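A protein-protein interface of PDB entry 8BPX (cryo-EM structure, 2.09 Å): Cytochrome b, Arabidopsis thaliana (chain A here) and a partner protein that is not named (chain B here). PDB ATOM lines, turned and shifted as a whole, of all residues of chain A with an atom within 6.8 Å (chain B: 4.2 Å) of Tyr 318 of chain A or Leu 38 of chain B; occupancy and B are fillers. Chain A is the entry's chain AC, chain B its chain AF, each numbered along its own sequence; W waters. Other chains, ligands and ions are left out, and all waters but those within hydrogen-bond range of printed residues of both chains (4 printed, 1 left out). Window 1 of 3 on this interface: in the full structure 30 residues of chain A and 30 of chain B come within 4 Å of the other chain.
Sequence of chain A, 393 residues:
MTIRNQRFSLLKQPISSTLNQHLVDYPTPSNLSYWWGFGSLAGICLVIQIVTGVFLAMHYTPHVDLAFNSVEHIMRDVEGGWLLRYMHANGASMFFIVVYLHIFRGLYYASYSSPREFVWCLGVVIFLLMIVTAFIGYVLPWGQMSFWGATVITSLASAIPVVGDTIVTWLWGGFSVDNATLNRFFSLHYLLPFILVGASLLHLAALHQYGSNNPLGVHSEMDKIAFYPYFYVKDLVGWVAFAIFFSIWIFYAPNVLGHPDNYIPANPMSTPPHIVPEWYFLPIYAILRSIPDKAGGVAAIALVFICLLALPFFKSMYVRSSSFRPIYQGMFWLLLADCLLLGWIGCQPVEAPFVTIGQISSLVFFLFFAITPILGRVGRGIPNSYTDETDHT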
ATOM      1  N   LEU A 216       8.355   3.775   0.987  1.00  0.00           N
ATOM      2  CA  LEU A 216       8.504   2.394   0.541  1.00  0.00           C
ATOM      3  C   LEU A 216       8.225   2.227  -0.945  1.00  0.00           C
ATOM      4  O   LEU A 216       8.639   1.222  -1.529  1.00  0.00           O
ATOM      5  CB  LEU A 216       7.582   1.477   1.348  1.00  0.00           C
ATOM      6  CG  LEU A 216       7.855   1.383   2.851  1.00  0.00           C
ATOM      7  CD1 LEU A 216       6.822   0.501   3.527  1.00  0.00           C
ATOM      8  CD2 LEU A 216       9.265   0.879   3.126  1.00  0.00           C
ATOM      9  N   GLY A 217       7.536   3.183  -1.565  1.00  0.00           N
ATOM     10  CA  GLY A 217       7.206   3.086  -2.971  1.00  0.00           C
ATOM     11  C   GLY A 217       6.132   2.080  -3.311  1.00  0.00           C
ATOM     12  O   GLY A 217       5.972   1.748  -4.486  1.00  0.00           O
ATOM     13  N   VAL A 218       5.380   1.600  -2.330  1.00  0.00           N
ATOM     14  CA  VAL A 218       4.425   0.531  -2.536  1.00  0.00           C
ATOM     15  C   VAL A 218       3.017   1.109  -2.611  1.00  0.00           C
ATOM     16  O   VAL A 218       2.788   2.284  -2.338  1.00  0.00           O
ATOM     17  CB  VAL A 218       4.516  -0.544  -1.424  1.00  0.00           C
ATOM     18  CG1 VAL A 218       5.897  -1.166  -1.388  1.00  0.00           C
ATOM     19  CG2 VAL A 218       4.138   0.054  -0.074  1.00  0.00           C
ATOM     20  N   HIS A 219       2.062   0.271  -3.003  1.00  0.00           N
ATOM     21  CA  HIS A 219       0.652   0.615  -2.888  1.00  0.00           C
ATOM     22  C   HIS A 219       0.303   0.882  -1.428  1.00  0.00           C
ATOM     23  O   HIS A 219       0.651   0.097  -0.543  1.00  0.00           O
ATOM     24  CB  HIS A 219      -0.199  -0.523  -3.450  1.00  0.00           C
ATOM     25  CG  HIS A 219      -1.545  -0.091  -3.942  1.00  0.00           C
ATOM     26  ND1 HIS A 219      -1.708   0.903  -4.880  1.00  0.00           N
ATOM     27  CD2 HIS A 219      -2.790  -0.524  -3.628  1.00  0.00           C
ATOM     28  CE1 HIS A 219      -2.995   1.072  -5.120  1.00  0.00           C
ATOM     29  NE2 HIS A 219      -3.674   0.216  -4.377  1.00  0.00           N
ATOM     30  N   SER A 316      10.647   1.571 -17.499  1.00  0.00           N
ATOM     31  CA  SER A 316      11.452   1.312 -16.321  1.00  0.00           C
ATOM     32  C   SER A 316      11.011   0.006 -15.680  1.00  0.00           C
ATOM     33  O   SER A 316      10.030  -0.619 -16.088  1.00  0.00           O
ATOM     34  CB  SER A 316      11.343   2.463 -15.313  1.00  0.00           C
ATOM     35  OG  SER A 316      10.132   2.393 -14.585  1.00  0.00           O
ATOM     36  N   MET A 317      11.768  -0.410 -14.672  1.00  0.00           N
ATOM     37  CA  MET A 317      11.316  -1.485 -13.816  1.00  0.00           C
ATOM     38  C   MET A 317      10.137  -0.999 -12.975  1.00  0.00           C
ATOM     39  O   MET A 317       9.828   0.192 -12.913  1.00  0.00           O
ATOM     40  CB  MET A 317      12.454  -1.981 -12.922  1.00  0.00           C
ATOM     41  CG  MET A 317      12.924  -0.965 -11.890  1.00  0.00           C
ATOM     42  SD  MET A 317      14.624  -1.238 -11.351  1.00  0.00           S
ATOM     43  CE  MET A 317      14.433  -2.677 -10.311  1.00  0.00           C
ATOM     44  N   TYR A 318       9.474  -1.945 -12.326  1.00  0.00           N
ATOM     45  CA  TYR A 318       8.268  -1.658 -11.566  1.00  0.00           C
ATOM     46  C   TYR A 318       8.553  -1.343 -10.106  1.00  0.00           C
ATOM     47  O   TYR A 318       7.628  -1.355  -9.291  1.00  0.00           O
ATOM     48  CB  TYR A 318       7.305  -2.840 -11.679  1.00  0.00           C
ATOM     49  CG  TYR A 318       7.019  -3.219 -13.112  1.00  0.00           C
ATOM     50  CD1 TYR A 318       6.023  -2.578 -13.833  1.00  0.00           C
ATOM     51  CD2 TYR A 318       7.761  -4.204 -13.752  1.00  0.00           C
ATOM     52  CE1 TYR A 318       5.761  -2.915 -15.145  1.00  0.00           C
ATOM     53  CE2 TYR A 318       7.508  -4.548 -15.064  1.00  0.00           C
ATOM     54  CZ  TYR A 318       6.506  -3.900 -15.755  1.00  0.00           C
ATOM     55  OH  TYR A 318       6.250  -4.239 -17.062  1.00  0.00           O
ATOM     56  N   VAL A 319       9.805  -1.069  -9.757  1.00  0.00           N
ATOM     57  CA  VAL A 319      10.200  -0.749  -8.393  1.00  0.00           C
ATOM     58  C   VAL A 319      10.557   0.728  -8.335  1.00  0.00           C
ATOM     59  O   VAL A 319      11.377   1.203  -9.128  1.00  0.00           O
ATOM     60  CB  VAL A 319      11.375  -1.626  -7.926  1.00  0.00           C
ATOM     61  CG1 VAL A 319      11.741  -1.298  -6.493  1.00  0.00           C
ATOM     62  CG2 VAL A 319      11.028  -3.101  -8.079  1.00  0.00           C
ATOM     63  N   ARG A 320       9.945   1.448  -7.398  1.00  0.00           N
ATOM     64  CA  ARG A 320      10.103   2.897  -7.320  1.00  0.00           C
ATOM     65  C   ARG A 320      11.244   3.313  -6.393  1.00  0.00           C
ATOM     66  O   ARG A 320      12.196   3.968  -6.825  1.00  0.00           O
ATOM     67  CB  ARG A 320       8.792   3.541  -6.853  1.00  0.00           C
ATOM     68  CG  ARG A 320       7.684   3.564  -7.885  1.00  0.00           C
ATOM     69  CD  ARG A 320       6.583   4.527  -7.470  1.00  0.00           C
ATOM     70  NE  ARG A 320       5.372   4.366  -8.265  1.00  0.00           N
ATOM     71  CZ  ARG A 320       4.316   3.659  -7.889  1.00  0.00           C
ATOM     72  NH1 ARG A 320       4.289   3.017  -6.734  1.00  0.00           N
ATOM     73  NH2 ARG A 320       3.261   3.592  -8.695  1.00  0.00           N
ATOM     74  N   PHE A 324      14.995   0.118  -2.147  1.00  0.00           N
ATOM     75  CA  PHE A 324      15.087  -1.241  -2.659  1.00  0.00           C
ATOM     76  C   PHE A 324      15.839  -1.324  -3.984  1.00  0.00           C
ATOM     77  O   PHE A 324      15.799  -2.369  -4.642  1.00  0.00           O
ATOM     78  CB  PHE A 324      13.685  -1.845  -2.796  1.00  0.00           C
ATOM     79  CG  PHE A 324      12.900  -1.848  -1.514  1.00  0.00           C
ATOM     80  CD1 PHE A 324      13.289  -2.646  -0.452  1.00  0.00           C
ATOM     81  CD2 PHE A 324      11.780  -1.046  -1.368  1.00  0.00           C
ATOM     82  CE1 PHE A 324      12.574  -2.649   0.731  1.00  0.00           C
ATOM     83  CE2 PHE A 324      11.059  -1.044  -0.187  1.00  0.00           C
ATOM     84  CZ  PHE A 324      11.454  -1.846   0.863  1.00  0.00           C
ATOM     85  N   GLY A 376      16.352   0.391 -15.773  1.00  0.00           N
ATOM     86  CA  GLY A 376      15.006  -0.162 -15.738  1.00  0.00           C
ATOM     87  C   GLY A 376      14.859  -1.396 -16.606  1.00  0.00           C
ATOM     88  O   GLY A 376      14.310  -2.419 -16.176  1.00  0.00           O
ATOM     89  N   GLY A 379      16.820  -4.294 -14.906  1.00  0.00           N
ATOM     90  CA  GLY A 379      16.203  -4.701 -13.661  1.00  0.00           C
ATOM     91  C   GLY A 379      14.826  -5.296 -13.810  1.00  0.00           C
ATOM     92  O   GLY A 379      14.320  -5.884 -12.849  1.00  0.00           O
ATOM     93  N   ARG A 380      14.206  -5.151 -14.984  1.00  0.00           N
ATOM     94  CA  ARG A 380      12.982  -5.894 -15.260  1.00  0.00           C
ATOM     95  C   ARG A 380      13.180  -7.395 -15.070  1.00  0.00           C
ATOM     96  O   ARG A 380      12.244  -8.099 -14.676  1.00  0.00           O
ATOM     97  CB  ARG A 380      12.501  -5.594 -16.681  1.00  0.00           C
ATOM     98  CG  ARG A 380      11.308  -6.412 -17.138  1.00  0.00           C
ATOM     99  CD  ARG A 380      10.852  -5.986 -18.528  1.00  0.00           C
ATOM    100  NE  ARG A 380       9.765  -6.817 -19.031  1.00  0.00           N
ATOM    101  CZ  ARG A 380       9.075  -6.558 -20.133  1.00  0.00           C
ATOM    102  NH1 ARG A 380       9.329  -5.491 -20.873  1.00  0.00           N
ATOM    103  NH2 ARG A 380       8.105  -7.389 -20.502  1.00  0.00           N
ATOM    104  N   LEU B  28      14.274  -6.137   2.201  1.00  0.00           N
ATOM    105  CA  LEU B  28      12.899  -6.627   2.218  1.00  0.00           C
ATOM    106  C   LEU B  28      12.574  -7.337   3.526  1.00  0.00           C
ATOM    107  O   LEU B  28      11.475  -7.180   4.069  1.00  0.00           O
ATOM    108  CB  LEU B  28      12.659  -7.565   1.039  1.00  0.00           C
ATOM    109  CG  LEU B  28      12.549  -6.958  -0.360  1.00  0.00           C
ATOM    110  CD1 LEU B  28      12.711  -8.045  -1.405  1.00  0.00           C
ATOM    111  CD2 LEU B  28      11.227  -6.230  -0.531  1.00  0.00           C
ATOM    112  N   LEU B  33       8.454  -7.670   3.802  1.00  0.00           N
ATOM    113  CA  LEU B  33       7.891  -7.564   2.468  1.00  0.00           C
ATOM    114  C   LEU B  33       8.496  -8.591   1.524  1.00  0.00           C
ATOM    115  O   LEU B  33       9.669  -8.955   1.630  1.00  0.00           O
ATOM    116  CB  LEU B  33       8.120  -6.167   1.895  1.00  0.00           C
ATOM    117  CG  LEU B  33       7.236  -5.042   2.424  1.00  0.00           C
ATOM    118  CD1 LEU B  33       7.728  -3.702   1.901  1.00  0.00           C
ATOM    119  CD2 LEU B  33       5.777  -5.282   2.064  1.00  0.00           C
ATOM    120  N   ARG B  34       7.682  -9.040   0.582  1.00  0.00           N
ATOM    121  CA  ARG B  34       8.161  -9.829  -0.539  1.00  0.00           C
ATOM    122  C   ARG B  34       8.458  -8.909  -1.715  1.00  0.00           C
ATOM    123  O   ARG B  34       7.885  -7.825  -1.835  1.00  0.00           O
ATOM    124  CB  ARG B  34       7.130 -10.884  -0.927  1.00  0.00           C
ATOM    125  CG  ARG B  34       6.970 -11.937   0.144  1.00  0.00           C
ATOM    126  CD  ARG B  34       6.372 -13.195  -0.392  1.00  0.00           C
ATOM    127  NE  ARG B  34       5.650 -13.937   0.629  1.00  0.00           N
ATOM    128  CZ  ARG B  34       5.032 -15.087   0.404  1.00  0.00           C
ATOM    129  NH1 ARG B  34       5.032 -15.645  -0.795  1.00  0.00           N
ATOM    130  NH2 ARG B  34       4.409 -15.695   1.408  1.00  0.00           N
ATOM    131  N   TYR B  35       9.372  -9.349  -2.584  1.00  0.00           N
ATOM    132  CA  TYR B  35       9.710  -8.544  -3.754  1.00  0.00           C
ATOM    133  C   TYR B  35       8.480  -8.277  -4.613  1.00  0.00           C
ATOM    134  O   TYR B  35       8.325  -7.181  -5.158  1.00  0.00           O
ATOM    135  CB  TYR B  35      10.798  -9.223  -4.579  1.00  0.00           C
ATOM    136  CG  TYR B  35      11.431  -8.297  -5.586  1.00  0.00           C
ATOM    137  CD1 TYR B  35      12.416  -7.396  -5.206  1.00  0.00           C
ATOM    138  CD2 TYR B  35      11.016  -8.292  -6.909  1.00  0.00           C
ATOM    139  CE1 TYR B  35      12.989  -6.539  -6.120  1.00  0.00           C
ATOM    140  CE2 TYR B  35      11.579  -7.438  -7.829  1.00  0.00           C
ATOM    141  CZ  TYR B  35      12.565  -6.562  -7.430  1.00  0.00           C
ATOM    142  OH  TYR B  35      13.127  -5.712  -8.346  1.00  0.00           O
ATOM    143  N   ASP B  36       7.592  -9.264  -4.734  1.00  0.00           N
ATOM    144  CA  ASP B  36       6.354  -9.074  -5.477  1.00  0.00           C
ATOM    145  C   ASP B  36       5.430  -8.050  -4.825  1.00  0.00           C
ATOM    146  O   ASP B  36       4.618  -7.441  -5.527  1.00  0.00           O
ATOM    147  CB  ASP B  36       5.624 -10.408  -5.635  1.00  0.00           C
ATOM    148  CG  ASP B  36       6.244 -11.291  -6.697  1.00  0.00           C
ATOM    149  OD1 ASP B  36       7.195 -10.845  -7.366  1.00  0.00           O
ATOM    150  OD2 ASP B  36       5.780 -12.435  -6.861  1.00  0.00           O
ATOM    151  N   ASP B  37       5.535  -7.847  -3.509  1.00  0.00           N
ATOM    152  CA  ASP B  37       4.751  -6.812  -2.841  1.00  0.00           C
ATOM    153  C   ASP B  37       5.111  -5.412  -3.327  1.00  0.00           C
ATOM    154  O   ASP B  37       4.290  -4.499  -3.207  1.00  0.00           O
ATOM    155  CB  ASP B  37       4.937  -6.887  -1.324  1.00  0.00           C
ATOM    156  CG  ASP B  37       4.439  -8.189  -0.733  1.00  0.00           C
ATOM    157  OD1 ASP B  37       3.522  -8.803  -1.312  1.00  0.00           O
ATOM    158  OD2 ASP B  37       4.973  -8.603   0.313  1.00  0.00           O
ATOM    159  N   LEU B  38       6.314  -5.224  -3.869  1.00  0.00           N
ATOM    160  CA  LEU B  38       6.712  -3.918  -4.375  1.00  0.00           C
ATOM    161  C   LEU B  38       6.023  -3.574  -5.689  1.00  0.00           C
ATOM    162  O   LEU B  38       6.060  -2.412  -6.104  1.00  0.00           O
ATOM    163  CB  LEU B  38       8.231  -3.858  -4.541  1.00  0.00           C
ATOM    164  CG  LEU B  38       9.053  -4.162  -3.285  1.00  0.00           C
ATOM    165  CD1 LEU B  38      10.537  -4.009  -3.568  1.00  0.00           C
ATOM    166  CD2 LEU B  38       8.630  -3.274  -2.120  1.00  0.00           C
ATOM    167  N   TYR B  39       5.453  -4.555  -6.370  1.00  0.00           N
ATOM    168  CA  TYR B  39       4.714  -4.358  -7.648  1.00  0.00           C
ATOM    169  C   TYR B  39       3.356  -3.736  -7.316  1.00  0.00           C
ATOM    170  O   TYR B  39       2.622  -4.281  -6.571  1.00  0.00           O
ATOM    171  CB  TYR B  39       4.750  -5.620  -8.510  1.00  0.00           C
ATOM    172  CG  TYR B  39       6.002  -5.952  -9.266  1.00  0.00           C
ATOM    173  CD1 TYR B  39       7.227  -6.044  -8.635  1.00  0.00           C
ATOM    174  CD2 TYR B  39       5.937  -6.258 -10.612  1.00  0.00           C
ATOM    175  CE1 TYR B  39       8.369  -6.369  -9.342  1.00  0.00           C
ATOM    176  CE2 TYR B  39       7.065  -6.587 -11.333  1.00  0.00           C
ATOM    177  CZ  TYR B  39       8.286  -6.642 -10.693  1.00  0.00           C
ATOM    178  OH  TYR B  39       9.404  -6.971 -11.383  1.00  0.00           O
ATOM    179  N   ASP B  40       3.105  -2.558  -7.808  1.00  0.00           N
ATOM    180  CA  ASP B  40       1.875  -1.787  -7.500  1.00  0.00           C
ATOM    181  C   ASP B  40       0.849  -1.836  -8.654  1.00  0.00           C
ATOM    182  O   ASP B  40       1.204  -1.564  -9.755  1.00  0.00           O
ATOM    183  CB  ASP B  40       2.285  -0.415  -6.944  1.00  0.00           C
ATOM    184  CG  ASP B  40       1.183   0.634  -6.829  1.00  0.00           C
ATOM    185  OD1 ASP B  40       0.032   0.285  -6.649  1.00  0.00           O
ATOM    186  OD2 ASP B  40       1.498   1.796  -6.913  1.00  0.00           O
ATOM    187  N   TYR B  43       0.894   1.286 -10.969  1.00  0.00           N
ATOM    188  CA  TYR B  43       1.993   1.442 -11.939  1.00  0.00           C
ATOM    189  C   TYR B  43       1.606   0.978 -13.350  1.00  0.00           C
ATOM    190  O   TYR B  43       1.964   1.608 -14.258  1.00  0.00           O
ATOM    191  CB  TYR B  43       3.296   0.766 -11.459  1.00  0.00           C
ATOM    192  CG  TYR B  43       4.460   0.923 -12.392  1.00  0.00           C
ATOM    193  CD1 TYR B  43       4.649   0.050 -13.444  1.00  0.00           C
ATOM    194  CD2 TYR B  43       5.355   1.960 -12.232  1.00  0.00           C
ATOM    195  CE1 TYR B  43       5.708   0.203 -14.315  1.00  0.00           C
ATOM    196  CE2 TYR B  43       6.411   2.138 -13.108  1.00  0.00           C
ATOM    197  CZ  TYR B  43       6.594   1.249 -14.147  1.00  0.00           C
ATOM    198  OH  TYR B  43       7.642   1.393 -15.006  1.00  0.00           O
ATOM    199  N   ILE B  47      -0.508  -5.246 -14.183  1.00  0.00           N
ATOM    200  CA  ILE B  47      -0.352  -5.685 -12.765  1.00  0.00           C
ATOM    201  C   ILE B  47      -1.718  -5.757 -12.116  1.00  0.00           C
ATOM    202  O   ILE B  47      -1.984  -6.768 -11.495  1.00  0.00           O
ATOM    203  CB  ILE B  47       0.699  -4.885 -11.926  1.00  0.00           C
ATOM    204  CG1 ILE B  47       2.110  -4.989 -12.508  1.00  0.00           C
ATOM    205  CG2 ILE B  47       0.653  -5.240 -10.447  1.00  0.00           C
ATOM    206  CD1 ILE B  47       3.057  -3.944 -11.981  1.00  0.00           C
ATOM    207  N   LYS B 102       0.718 -10.480 -19.882  1.00  0.00           N
ATOM    208  CA  LYS B 102       1.433  -9.770 -20.939  1.00  0.00           C
ATOM    209  C   LYS B 102       1.416 -10.557 -22.245  1.00  0.00           C
ATOM    210  O   LYS B 102       1.274  -9.971 -23.326  1.00  0.00           O
ATOM    211  CB  LYS B 102       2.866  -9.470 -20.499  1.00  0.00           C
ATOM    212  CG  LYS B 102       2.961  -8.373 -19.459  1.00  0.00           C
ATOM    213  CD  LYS B 102       4.135  -8.583 -18.529  1.00  0.00           C
ATOM    214  CE  LYS B 102       4.579  -7.281 -17.883  1.00  0.00           C
ATOM    215  NZ  LYS B 102       3.516  -6.234 -17.893  1.00  0.00           N
HETATM  216  O   HOH W   1       7.386   0.057  -5.904  1.00  0.00           O
HETATM  217  O   HOH W   2       2.995  -2.513  -3.968  1.00  0.00           O
HETATM  218  O   HOH W   3      11.900  -5.593 -11.021  1.00  0.00           O
HETATM  219  O   HOH W   4      15.545  -3.572  -7.070  1.00  0.00           O
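The backbone carbonyl oxygen (O) of Gly 217 of chain A sits at hydrogen-bond distance from the guanidinium group (NH1) of Arg 320 of chain A.
Of the 12 printed residues of chain B, 7 touch a printed residue of chain A. Printed residues of chain B that touch a printed residue of chain A: Tyr 35, Leu 38, Tyr 39, Asp 40, Tyr 43, Ile 47 and Lys 102. Along chain B the printed residues that touch a printed residue of chain A span positions 35 to 102. Printed residues of chain A that touch a printed residue of chain B: Val 218, His 219, Ser 316, Met 317, Tyr 318, Val 319, Arg 320 and Phe 324. Hydrophobic or aromatic side chains of chain A that line the printed part of chain B: Val 218, His 219, Met 317, Tyr 318, Val 319 and Phe 324. Among the printed residues, 14 pairs touch across the chains. Among the printed residues, Asp or Glu carboxylates within 4 Å of a Lys or Arg side-chain nitrogen of the other chain: Arg 320 of chain A with Asp 40 of chain B.
Water W2 lies within hydrogen-bond range of O of Asp 37 of chain B (2.5 Å), N of His 219 of chain A (3.1 Å) and O of Tyr 39 of chain B (3.2 Å). Water W1 lies within hydrogen-bond range of O of Gly 217 of chain A, O of Leu 38 of chain B and N of Arg 320 of chain A. Water W4 lies within hydrogen-bond range of O of Phe 324 of chain A and OH of Tyr 35 of chain B. Water W3 lies within hydrogen-bond range of the side-chain hydroxyl (OH) of Tyr 39 of chain B, the side-chain hydroxyl (OH) of Tyr 35 of chain B and the backbone carbonyl oxygen (O) of Gly 379 of chain A.
The backbone carbonyl oxygen (O) of Met 317 of chain A is in hydrogen-bond range of the side-chain hydroxyl (OH) of Tyr 43 of chain B (3.3 Å). OH of Tyr 318 of chain A sits at hydrogen-bond distance from NZ of Lys 102 of chain B (3.5 Å). A ring nitrogen (ND1) of His 219 of chain A sits at hydrogen-bond distance from the side-chain carboxylate (OD1) of Asp 40 of chain B, at 2.6 Å. The side-chain hydroxyl of Tyr 43 of chain B is in hydrogen-bond range of the side-chain hydroxyl of Ser 316 of chain A (2.7 Å). The side-chain carboxylate (OD2) of Asp 40 of chain B is in salt-bridge range of the guanidinium group (NH1) of Arg 320 of chain A (3.1 Å).
Of chain A, only Val 218, Tyr 318 and Phe 324 come within 4 Å of Leu 38 of chain B. Of the printed residues of chain A, Tyr 43 of chain B touches Ser 316 (2.7 Å), Met 317 (3.3 Å), Tyr 318 (2.8 Å) and Arg 320 (3.95 Å). Of the printed residues of chain A, Tyr 35 of chain B touches Met 317 (3.8 Å) and Val 319 (3.4 Å). Gly 217 of chain A touches none of the printed residues of chain B. Arg 34 of chain B touches none of the printed residues of chain A. The nearest residue of chain A that does not touch Leu 38 of chain B is Val 319 of chain A (4.2 Å).
Val 218 of chain A touches Leu 38 of chain B. Met 317 of chain A touches Tyr 35 of chain B (CE to OH, 3.8 Å). Tyr 318 of chain A touches Leu 38 of chain B. Tyr 318 of chain A touches Tyr 39 of chain B (CD2 to CE2, 3.5 Å). CD1 of Tyr 318 of chain A touches CE1 of Tyr 43 of chain B, 2.8 Å away. Tyr 318 of chain A touches Ile 47 of chain B (CD1 to CD1, 3.8 Å). OH of Tyr 35 of chain B touches CG2 of Val 319 of chain A, at 3.4 Å. CB of Tyr 43 of chain B touches NH2 of Arg 320 of chain A, 3.95 Å away. Phe 324 of chain A touches Leu 38 of chain B (CG to CD1, 3.8 Å).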
